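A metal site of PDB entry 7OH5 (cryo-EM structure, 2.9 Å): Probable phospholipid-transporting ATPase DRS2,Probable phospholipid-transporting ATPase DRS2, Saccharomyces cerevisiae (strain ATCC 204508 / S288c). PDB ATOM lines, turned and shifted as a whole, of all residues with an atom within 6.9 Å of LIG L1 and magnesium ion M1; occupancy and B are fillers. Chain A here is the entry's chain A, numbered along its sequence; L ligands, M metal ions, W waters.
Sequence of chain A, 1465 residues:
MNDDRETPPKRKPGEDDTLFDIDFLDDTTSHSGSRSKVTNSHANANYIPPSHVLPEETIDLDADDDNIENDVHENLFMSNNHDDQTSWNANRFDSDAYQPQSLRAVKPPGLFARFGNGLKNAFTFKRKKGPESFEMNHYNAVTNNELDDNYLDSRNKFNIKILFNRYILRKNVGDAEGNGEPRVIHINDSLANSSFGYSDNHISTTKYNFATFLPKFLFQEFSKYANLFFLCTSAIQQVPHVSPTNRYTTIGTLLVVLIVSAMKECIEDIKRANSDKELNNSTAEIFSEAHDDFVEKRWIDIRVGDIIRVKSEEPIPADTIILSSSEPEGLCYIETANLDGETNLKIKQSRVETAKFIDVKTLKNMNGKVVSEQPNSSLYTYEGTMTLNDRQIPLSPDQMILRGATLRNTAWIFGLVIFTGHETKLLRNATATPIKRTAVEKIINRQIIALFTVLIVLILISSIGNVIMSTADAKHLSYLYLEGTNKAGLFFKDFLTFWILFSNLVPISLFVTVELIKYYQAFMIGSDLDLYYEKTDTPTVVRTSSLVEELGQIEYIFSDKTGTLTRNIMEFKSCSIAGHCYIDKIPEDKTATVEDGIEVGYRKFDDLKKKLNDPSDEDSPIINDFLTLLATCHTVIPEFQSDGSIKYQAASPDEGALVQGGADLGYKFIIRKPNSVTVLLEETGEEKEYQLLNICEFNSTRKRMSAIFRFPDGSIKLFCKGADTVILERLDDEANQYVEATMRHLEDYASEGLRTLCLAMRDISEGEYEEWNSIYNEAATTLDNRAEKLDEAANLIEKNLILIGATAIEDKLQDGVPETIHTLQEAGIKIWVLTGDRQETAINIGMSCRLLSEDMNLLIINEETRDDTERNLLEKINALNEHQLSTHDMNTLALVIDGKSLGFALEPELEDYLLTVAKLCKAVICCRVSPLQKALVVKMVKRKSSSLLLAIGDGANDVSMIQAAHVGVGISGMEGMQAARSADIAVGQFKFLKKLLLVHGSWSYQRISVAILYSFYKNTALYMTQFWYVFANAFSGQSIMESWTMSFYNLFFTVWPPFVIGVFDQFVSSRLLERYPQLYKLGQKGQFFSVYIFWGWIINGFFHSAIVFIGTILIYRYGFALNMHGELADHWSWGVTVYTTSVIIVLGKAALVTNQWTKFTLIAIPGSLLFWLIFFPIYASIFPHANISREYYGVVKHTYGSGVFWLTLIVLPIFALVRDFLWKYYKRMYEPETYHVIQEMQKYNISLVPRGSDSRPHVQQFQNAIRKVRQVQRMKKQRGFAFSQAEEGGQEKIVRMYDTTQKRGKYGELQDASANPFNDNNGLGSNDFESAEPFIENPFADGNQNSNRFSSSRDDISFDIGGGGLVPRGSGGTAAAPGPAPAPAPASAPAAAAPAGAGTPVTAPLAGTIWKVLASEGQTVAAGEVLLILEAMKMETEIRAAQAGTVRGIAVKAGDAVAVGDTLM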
ATOM      1  N   SER A 559     -16.791  -2.344  18.164  1.00  0.00           N
ATOM      2  CA  SER A 559     -18.169  -2.448  17.703  1.00  0.00           C
ATOM      3  C   SER A 559     -18.245  -2.394  16.187  1.00  0.00           C
ATOM      4  O   SER A 559     -17.273  -2.680  15.473  1.00  0.00           O
ATOM      5  CB  SER A 559     -19.011  -1.350  18.348  1.00  0.00           C
ATOM      6  OG  SER A 559     -20.354  -1.416  17.906  1.00  0.00           O
ATOM      7  N   ASP A 560     -19.421  -2.032  15.670  1.00  0.00           N
ATOM      8  CA  ASP A 560     -19.694  -1.980  14.242  1.00  0.00           C
ATOM      9  C   ASP A 560     -20.926  -1.113  14.038  1.00  0.00           C
ATOM     10  O   ASP A 560     -21.770  -0.995  14.932  1.00  0.00           O
ATOM     11  CB  ASP A 560     -19.875  -3.396  13.672  1.00  0.00           C
ATOM     12  CG  ASP A 560     -20.697  -3.417  12.388  1.00  0.00           C
ATOM     13  OD1 ASP A 560     -20.236  -2.852  11.363  1.00  0.00           O
ATOM     14  OD2 ASP A 560     -21.793  -3.999  12.410  1.00  0.00           O
ATOM     15  N   LYS A 561     -21.023  -0.486  12.862  1.00  0.00           N
ATOM     16  CA  LYS A 561     -22.104   0.470  12.597  1.00  0.00           C
ATOM     17  C   LYS A 561     -23.354  -0.230  12.060  1.00  0.00           C
ATOM     18  O   LYS A 561     -24.390  -0.261  12.732  1.00  0.00           O
ATOM     19  CB  LYS A 561     -21.620   1.551  11.629  1.00  0.00           C
ATOM     20  CG  LYS A 561     -22.597   2.703  11.471  1.00  0.00           C
ATOM     21  CD  LYS A 561     -22.245   3.594  10.301  1.00  0.00           C
ATOM     22  CE  LYS A 561     -22.463   2.876   8.980  1.00  0.00           C
ATOM     23  NZ  LYS A 561     -22.209   3.771   7.812  1.00  0.00           N
ATOM     24  N   THR A 562     -23.265  -0.783  10.855  1.00  0.00           N
ATOM     25  CA  THR A 562     -24.433  -1.318  10.173  1.00  0.00           C
ATOM     26  C   THR A 562     -24.936  -2.575  10.884  1.00  0.00           C
ATOM     27  O   THR A 562     -24.224  -3.572  10.976  1.00  0.00           O
ATOM     28  CB  THR A 562     -24.100  -1.635   8.725  1.00  0.00           C
ATOM     29  OG1 THR A 562     -23.700  -0.436   8.048  1.00  0.00           O
ATOM     30  CG2 THR A 562     -25.309  -2.226   8.011  1.00  0.00           C
ATOM     31  N   GLY A 563     -26.157  -2.520  11.385  1.00  0.00           N
ATOM     32  CA  GLY A 563     -26.759  -3.650  12.069  1.00  0.00           C
ATOM     33  C   GLY A 563     -26.535  -3.679  13.565  1.00  0.00           C
ATOM     34  O   GLY A 563     -27.466  -3.917  14.331  1.00  0.00           O
ATOM     35  N   THR A 564     -25.292  -3.443  13.988  1.00  0.00           N
ATOM     36  CA  THR A 564     -24.981  -3.419  15.411  1.00  0.00           C
ATOM     37  C   THR A 564     -25.465  -2.137  16.068  1.00  0.00           C
ATOM     38  O   THR A 564     -26.091  -2.172  17.135  1.00  0.00           O
ATOM     39  CB  THR A 564     -23.478  -3.603  15.624  1.00  0.00           C
ATOM     40  OG1 THR A 564     -23.046  -4.827  15.020  1.00  0.00           O
ATOM     41  CG2 THR A 564     -23.143  -3.619  17.107  1.00  0.00           C
ATOM     42  N   LEU A 565     -25.201  -0.988  15.435  1.00  0.00           N
ATOM     43  CA  LEU A 565     -25.657   0.294  15.951  1.00  0.00           C
ATOM     44  C   LEU A 565     -26.932   0.783  15.282  1.00  0.00           C
ATOM     45  O   LEU A 565     -27.625   1.619  15.865  1.00  0.00           O
ATOM     46  CB  LEU A 565     -24.560   1.352  15.775  1.00  0.00           C
ATOM     47  CG  LEU A 565     -23.350   1.262  16.699  1.00  0.00           C
ATOM     48  CD1 LEU A 565     -22.302   2.295  16.311  1.00  0.00           C
ATOM     49  CD2 LEU A 565     -23.772   1.458  18.145  1.00  0.00           C
ATOM     50  N   THR A 566     -27.264   0.290  14.091  1.00  0.00           N
ATOM     51  CA  THR A 566     -28.442   0.706  13.355  1.00  0.00           C
ATOM     52  C   THR A 566     -29.398  -0.467  13.206  1.00  0.00           C
ATOM     53  O   THR A 566     -29.024  -1.630  13.367  1.00  0.00           O
ATOM     54  CB  THR A 566     -28.071   1.259  11.973  1.00  0.00           C
ATOM     55  OG1 THR A 566     -27.383   0.250  11.224  1.00  0.00           O
ATOM     56  CG2 THR A 566     -27.185   2.478  12.115  1.00  0.00           C
ATOM     57  N   ASN A 568     -30.635  -1.546  10.543  1.00  0.00           N
ATOM     58  CA  ASN A 568     -30.329  -2.230   9.295  1.00  0.00           C
ATOM     59  C   ASN A 568     -31.562  -2.413   8.411  1.00  0.00           C
ATOM     60  O   ASN A 568     -31.607  -3.333   7.587  1.00  0.00           O
ATOM     61  CB  ASN A 568     -29.653  -3.587   9.549  1.00  0.00           C
ATOM     62  CG  ASN A 568     -28.780  -4.029   8.402  1.00  0.00           C
ATOM     63  OD1 ASN A 568     -28.420  -3.232   7.536  1.00  0.00           O
ATOM     64  ND2 ASN A 568     -28.419  -5.312   8.387  1.00  0.00           N
ATOM     65  N   VAL A 833     -15.085   1.875  16.912  1.00  0.00           N
ATOM     66  CA  VAL A 833     -16.020   1.533  15.846  1.00  0.00           C
ATOM     67  C   VAL A 833     -15.209   1.195  14.596  1.00  0.00           C
ATOM     68  O   VAL A 833     -14.431   2.017  14.107  1.00  0.00           O
ATOM     69  CB  VAL A 833     -17.006   2.681  15.564  1.00  0.00           C
ATOM     70  CG1 VAL A 833     -18.034   2.251  14.535  1.00  0.00           C
ATOM     71  CG2 VAL A 833     -17.684   3.122  16.853  1.00  0.00           C
ATOM     72  N   LEU A 834     -15.390  -0.024  14.093  1.00  0.00           N
ATOM     73  CA  LEU A 834     -14.687  -0.516  12.913  1.00  0.00           C
ATOM     74  C   LEU A 834     -15.722  -0.705  11.805  1.00  0.00           C
ATOM     75  O   LEU A 834     -16.307  -1.780  11.640  1.00  0.00           O
ATOM     76  CB  LEU A 834     -13.947  -1.821  13.203  1.00  0.00           C
ATOM     77  CG  LEU A 834     -12.632  -1.750  13.986  1.00  0.00           C
ATOM     78  CD1 LEU A 834     -12.871  -1.446  15.462  1.00  0.00           C
ATOM     79  CD2 LEU A 834     -11.846  -3.039  13.830  1.00  0.00           C
ATOM     80  N   THR A 835     -15.947   0.363  11.030  1.00  0.00           N
ATOM     81  CA  THR A 835     -16.950   0.371   9.981  1.00  0.00           C
ATOM     82  C   THR A 835     -16.284   0.256   8.618  1.00  0.00           C
ATOM     83  O   THR A 835     -15.214   0.840   8.383  1.00  0.00           O
ATOM     84  CB  THR A 835     -17.784   1.659  10.043  1.00  0.00           C
ATOM     85  OG1 THR A 835     -18.283   1.831  11.368  1.00  0.00           O
ATOM     86  CG2 THR A 835     -18.949   1.582   9.068  1.00  0.00           C
ATOM     87  N   GLY A 836     -16.910  -0.490   7.720  1.00  0.00           N
ATOM     88  CA  GLY A 836     -16.461  -0.600   6.345  1.00  0.00           C
ATOM     89  C   GLY A 836     -17.095   0.387   5.389  1.00  0.00           C
ATOM     90  O   GLY A 836     -16.911   0.258   4.176  1.00  0.00           O
ATOM     91  N   ASP A 837     -17.828   1.369   5.894  1.00  0.00           N
ATOM     92  CA  ASP A 837     -18.528   2.343   5.086  1.00  0.00           C
ATOM     93  C   ASP A 837     -17.718   3.640   4.999  1.00  0.00           C
ATOM     94  O   ASP A 837     -16.509   3.644   5.284  1.00  0.00           O
ATOM     95  CB  ASP A 837     -19.936   2.560   5.670  1.00  0.00           C
ATOM     96  CG  ASP A 837     -20.919   3.103   4.641  1.00  0.00           C
ATOM     97  OD1 ASP A 837     -20.584   3.110   3.439  1.00  0.00           O
ATOM     98  OD2 ASP A 837     -22.020   3.526   5.045  1.00  0.00           O
ATOM     99  N   VAL A 929     -12.860  -0.109   6.655  1.00  0.00           N
ATOM    100  CA  VAL A 929     -12.010  -1.172   7.172  1.00  0.00           C
ATOM    101  C   VAL A 929     -12.314  -2.463   6.434  1.00  0.00           C
ATOM    102  O   VAL A 929     -13.481  -2.835   6.260  1.00  0.00           O
ATOM    103  CB  VAL A 929     -12.205  -1.345   8.686  1.00  0.00           C
ATOM    104  CG1 VAL A 929     -11.171  -2.293   9.254  1.00  0.00           C
ATOM    105  CG2 VAL A 929     -12.128   0.000   9.382  1.00  0.00           C
ATOM    106  N   LYS A 934     -10.146  -5.872  10.253  1.00  0.00           N
ATOM    107  CA  LYS A 934     -10.859  -5.790  11.527  1.00  0.00           C
ATOM    108  C   LYS A 934     -10.233  -6.705  12.571  1.00  0.00           C
ATOM    109  O   LYS A 934     -10.380  -6.467  13.774  1.00  0.00           O
ATOM    110  CB  LYS A 934     -12.334  -6.138  11.336  1.00  0.00           C
ATOM    111  CG  LYS A 934     -13.123  -5.124  10.525  1.00  0.00           C
ATOM    112  CD  LYS A 934     -14.591  -5.491  10.464  1.00  0.00           C
ATOM    113  CE  LYS A 934     -15.411  -4.388   9.822  1.00  0.00           C
ATOM    114  NZ  LYS A 934     -16.865  -4.702   9.819  1.00  0.00           N
ATOM    115  N   GLY A 953     -20.618  -7.642  16.823  1.00  0.00           N
ATOM    116  CA  GLY A 953     -20.927  -7.324  15.441  1.00  0.00           C
ATOM    117  C   GLY A 953     -21.883  -8.334  14.853  1.00  0.00           C
ATOM    118  O   GLY A 953     -22.288  -9.303  15.500  1.00  0.00           O
ATOM    119  N   ASP A 954     -22.230  -8.099  13.589  1.00  0.00           N
ATOM    120  CA  ASP A 954     -23.154  -8.957  12.854  1.00  0.00           C
ATOM    121  C   ASP A 954     -22.665  -9.118  11.430  1.00  0.00           C
ATOM    122  O   ASP A 954     -22.057  -8.208  10.861  1.00  0.00           O
ATOM    123  CB  ASP A 954     -24.581  -8.392  12.870  1.00  0.00           C
ATOM    124  CG  ASP A 954     -24.689  -7.053  12.169  1.00  0.00           C
ATOM    125  OD1 ASP A 954     -23.684  -6.292  12.138  1.00  0.00           O
ATOM    126  OD2 ASP A 954     -25.774  -6.740  11.654  1.00  0.00           O
ATOM    127  N   GLY A 955     -22.930 -10.279  10.853  1.00  0.00           N
ATOM    128  CA  GLY A 955     -22.552 -10.560   9.484  1.00  0.00           C
ATOM    129  C   GLY A 955     -21.223 -11.293   9.387  1.00  0.00           C
ATOM    130  O   GLY A 955     -20.497 -11.469  10.365  1.00  0.00           O
ATOM    131  N   ASN A 957     -18.587 -10.311   7.862  1.00  0.00           N
ATOM    132  CA  ASN A 957     -17.434  -9.439   7.723  1.00  0.00           C
ATOM    133  C   ASN A 957     -16.675  -9.249   9.031  1.00  0.00           C
ATOM    134  O   ASN A 957     -15.463  -9.027   9.000  1.00  0.00           O
ATOM    135  CB  ASN A 957     -17.857  -8.074   7.163  1.00  0.00           C
ATOM    136  CG  ASN A 957     -18.877  -7.384   8.045  1.00  0.00           C
ATOM    137  OD1 ASN A 957     -18.515  -6.684   8.996  1.00  0.00           O
ATOM    138  ND2 ASN A 957     -20.154  -7.558   7.725  1.00  0.00           N
ATOM    139  N   ASP A 958     -17.357  -9.337  10.163  1.00  0.00           N
ATOM    140  CA  ASP A 958     -16.723  -9.216  11.477  1.00  0.00           C
ATOM    141  C   ASP A 958     -16.791 -10.528  12.255  1.00  0.00           C
ATOM    142  O   ASP A 958     -17.024 -10.550  13.462  1.00  0.00           O
ATOM    143  CB  ASP A 958     -17.345  -8.085  12.285  1.00  0.00           C
ATOM    144  CG  ASP A 958     -18.858  -8.178  12.358  1.00  0.00           C
ATOM    145  OD1 ASP A 958     -19.377  -9.063  13.057  1.00  0.00           O
ATOM    146  OD2 ASP A 958     -19.527  -7.343  11.716  1.00  0.00           O
ATOM    147  N   MET A 961     -13.210 -10.671  13.725  1.00  0.00           N
ATOM    148  CA  MET A 961     -13.112  -9.749  14.861  1.00  0.00           C
ATOM    149  C   MET A 961     -13.594 -10.406  16.145  1.00  0.00           C
ATOM    150  O   MET A 961     -13.058 -10.138  17.227  1.00  0.00           O
ATOM    151  CB  MET A 961     -13.924  -8.486  14.570  1.00  0.00           C
ATOM    152  CG  MET A 961     -13.939  -7.478  15.705  1.00  0.00           C
ATOM    153  SD  MET A 961     -15.341  -6.350  15.630  1.00  0.00           S
ATOM    154  CE  MET A 961     -15.072  -5.592  14.038  1.00  0.00           C
ATOM    155  N   GLU A 975     -28.578  -9.688   8.367  1.00  0.00           N
ATOM    156  CA  GLU A 975     -27.487 -10.153   7.519  1.00  0.00           C
ATOM    157  C   GLU A 975     -27.328 -11.665   7.510  1.00  0.00           C
ATOM    158  O   GLU A 975     -26.646 -12.195   6.630  1.00  0.00           O
ATOM    159  CB  GLU A 975     -26.168  -9.492   7.950  1.00  0.00           C
ATOM    160  CG  GLU A 975     -26.117  -7.993   7.732  1.00  0.00           C
ATOM    161  CD  GLU A 975     -26.077  -7.617   6.258  1.00  0.00           C
ATOM    162  OE1 GLU A 975     -25.694  -8.479   5.429  1.00  0.00           O
ATOM    163  OE2 GLU A 975     -26.432  -6.470   5.924  1.00  0.00           O
HETATM  164 AL1  LIG L   1     -20.264  -3.072   9.672  1.00  0.00          AL
HETATM  165  F1  LIG L   1     -20.875  -1.617  10.474  1.00  0.00           F
HETATM  166  F2  LIG L   1     -19.674  -4.553   8.818  1.00  0.00           F
HETATM  167  F3  LIG L   1     -18.636  -2.346   9.542  1.00  0.00           F
HETATM  168  F4  LIG L   1     -21.893  -3.804   9.780  1.00  0.00           F
HETATM  169  P1  LG2 L   2     -20.969  -2.117   6.819  1.00  0.00           P
HETATM  170  O1  LG2 L   2     -20.366  -2.793   7.995  1.00  0.00           O
HETATM  171  O2  LG2 L   2     -21.413  -0.705   7.210  1.00  0.00           O
HETATM  172  O3  LG2 L   2     -22.150  -2.899   6.345  1.00  0.00           O
HETATM  173  P2  LG2 L   2     -19.567  -3.139   4.432  1.00  0.00           P
HETATM  174  O4  LG2 L   2     -18.668  -4.232   4.995  1.00  0.00           O
HETATM  175  O5  LG2 L   2     -20.859  -3.733   3.977  1.00  0.00           O
HETATM  176  O6  LG2 L   2     -19.844  -2.006   5.579  1.00  0.00           O
HETATM  177  O7  LG2 L   2     -18.792  -2.408   3.136  1.00  0.00           O
HETATM  178  C1  LG2 L   2     -19.347  -2.579   1.815  1.00  0.00           C
HETATM  179  C2  LG2 L   2     -19.592  -1.152   1.162  1.00  0.00           C
HETATM  180  O8  LG2 L   2     -19.940  -1.337  -0.344  1.00  0.00           O
HETATM  181  C3  LG2 L   2     -20.602  -0.602   1.715  1.00  0.00           C
HETATM  182  O9  LG2 L   2     -20.182   0.534   2.523  1.00  0.00           O
HETATM  183  C4  LG2 L   2     -21.602  -0.071   0.500  1.00  0.00           C
HETATM  184  O10 LG2 L   2     -21.298   1.306   0.159  1.00  0.00           O
HETATM  185  C5  LG2 L   2     -21.391  -0.830  -0.511  1.00  0.00           C
HETATM  186  N1  LG2 L   2     -22.345  -1.980  -0.489  1.00  0.00           N
HETATM  187  C6  LG2 L   2     -23.168  -2.503   0.429  1.00  0.00           C
HETATM  188  N2  LG2 L   2     -23.792  -3.556  -0.171  1.00  0.00           N
HETATM  189  C7  LG2 L   2     -23.341  -3.650  -1.438  1.00  0.00           C
HETATM  190  C8  LG2 L   2     -23.634  -4.512  -2.476  1.00  0.00           C
HETATM  191  N3  LG2 L   2     -24.577  -5.664  -2.520  1.00  0.00           N
HETATM  192  N4  LG2 L   2     -23.015  -4.369  -3.688  1.00  0.00           N
HETATM  193  C9  LG2 L   2     -22.112  -3.374  -3.872  1.00  0.00           C
HETATM  194  N5  LG2 L   2     -21.819  -2.520  -2.846  1.00  0.00           N
HETATM  195  C10 LG2 L   2     -22.433  -2.649  -1.643  1.00  0.00           C
HETATM  196 MG    MG M   1     -22.697  -4.909  10.827  1.00  0.00          MG
HETATM  197 MG    MG M   2     -21.963  -5.451   4.222  1.00  0.00          MG
HETATM  198  O   HOH W   1     -23.611  -5.811   9.197  1.00  0.00           O
HETATM  199  O   HOH W   2     -21.141  -6.195  10.630  1.00  0.00           O
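N of Thr 566 is in hydrogen-bond range of O of Lys 561, 3.2 Å away.
The backbone NH (N) of Leu 565 sits close to the backbone carbonyl oxygen (O) of Asp 560, at 3.5 Å.
O of Thr 835 sits at hydrogen-bond distance from N of Val 929 (3.1 Å).
The side-chain carboxylate (OD1) of Asp 958 lies within hydrogen-bond range of the backbone NH (N) of Asp 954, 3.1 Å away.
OD2 of Asp 560 sits close to OG1 of Thr 564.
The side-chain amide oxygen (OD1) of Asn 957 lies close to the side-chain carboxylate (OD2) of Asp 958, 3.0 Å away.
The side-chain carboxylate (OD1) of Asp 954 sits close to the side-chain hydroxyl (OG1) of Thr 564 (3.3 Å).
The side-chain amino group (NZ) of Lys 561 is in salt-bridge range of the side-chain carboxylate (OD2) of Asp 837, 2.8 Å away.
A fluorine (F4) of LIG L1 binds magnesium ion M1.
Water W2 is bound to magnesium ion M1 (2.0 Å).
O of Thr 562 binds magnesium ion M1, 2.0 Å away.
Magnesium ion M1 is bound by OD2 of Asp 560 (2.0 Å).
Magnesium ion M1 is bound by water W1 (2.1 Å).
Magnesium ion M1 is bound by the side-chain carboxylate (OD1) of Asp 954 (2.1 Å).
The side-chain carboxylate (OD1) of Asp 560 binds an aluminium atom (AL1) of LIG L1, 1.7 Å away.
The backbone NH (N) of Lys 561 lies within hydrogen-bond range of a fluorine (F1) of LIG L1, at 2.6 Å.
N of Gly 836 is in hydrogen-bond range of F3 of LIG L1, at 3.1 Å.
The side-chain carboxylate (OD1) of Asp 837 sits at hydrogen-bond distance from an oxygen (O9) of LG2 L2 (2.8 Å).
O2 of LG2 L2 is in hydrogen-bond range of OG1 of Thr 562 (2.5 Å).
F3 of LIG L1 sits at hydrogen-bond distance from NZ of Lys 934 (3.0 Å).
The side-chain amide oxygen (OD1) of Asn 957 lies close to a fluorine (F2) of LIG L1 (2.4 Å).
N of Thr 562 is in hydrogen-bond range of F1 of LIG L1, at 2.6 Å.
Within 4 Å of magnesium ion M1: Asp 560, Thr 562 and Asp 954.
The nearest printed residue that does not touch magnesium ion M1 is Asp 958 (4.1 Å).
The backbone carbonyl oxygen (O) of Leu 834 sits close to a fluorine (F3) of LIG L1 (3.2 Å).
Thr 835 touches LIG L1.
Nine residues have an atom within 4 Å of LIG L1: Asp 560, Lys 561, Thr 562, Leu 834, Thr 835, Gly 836, Lys 934, Asp 954 and Asn 957.
The nearest printed residue that does not touch LIG L1 is Asp 958 (4.03 Å).
An oxygen (O1) of LG2 L2 binds an aluminium atom (AL1) of LIG L1, at 1.7 Å.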
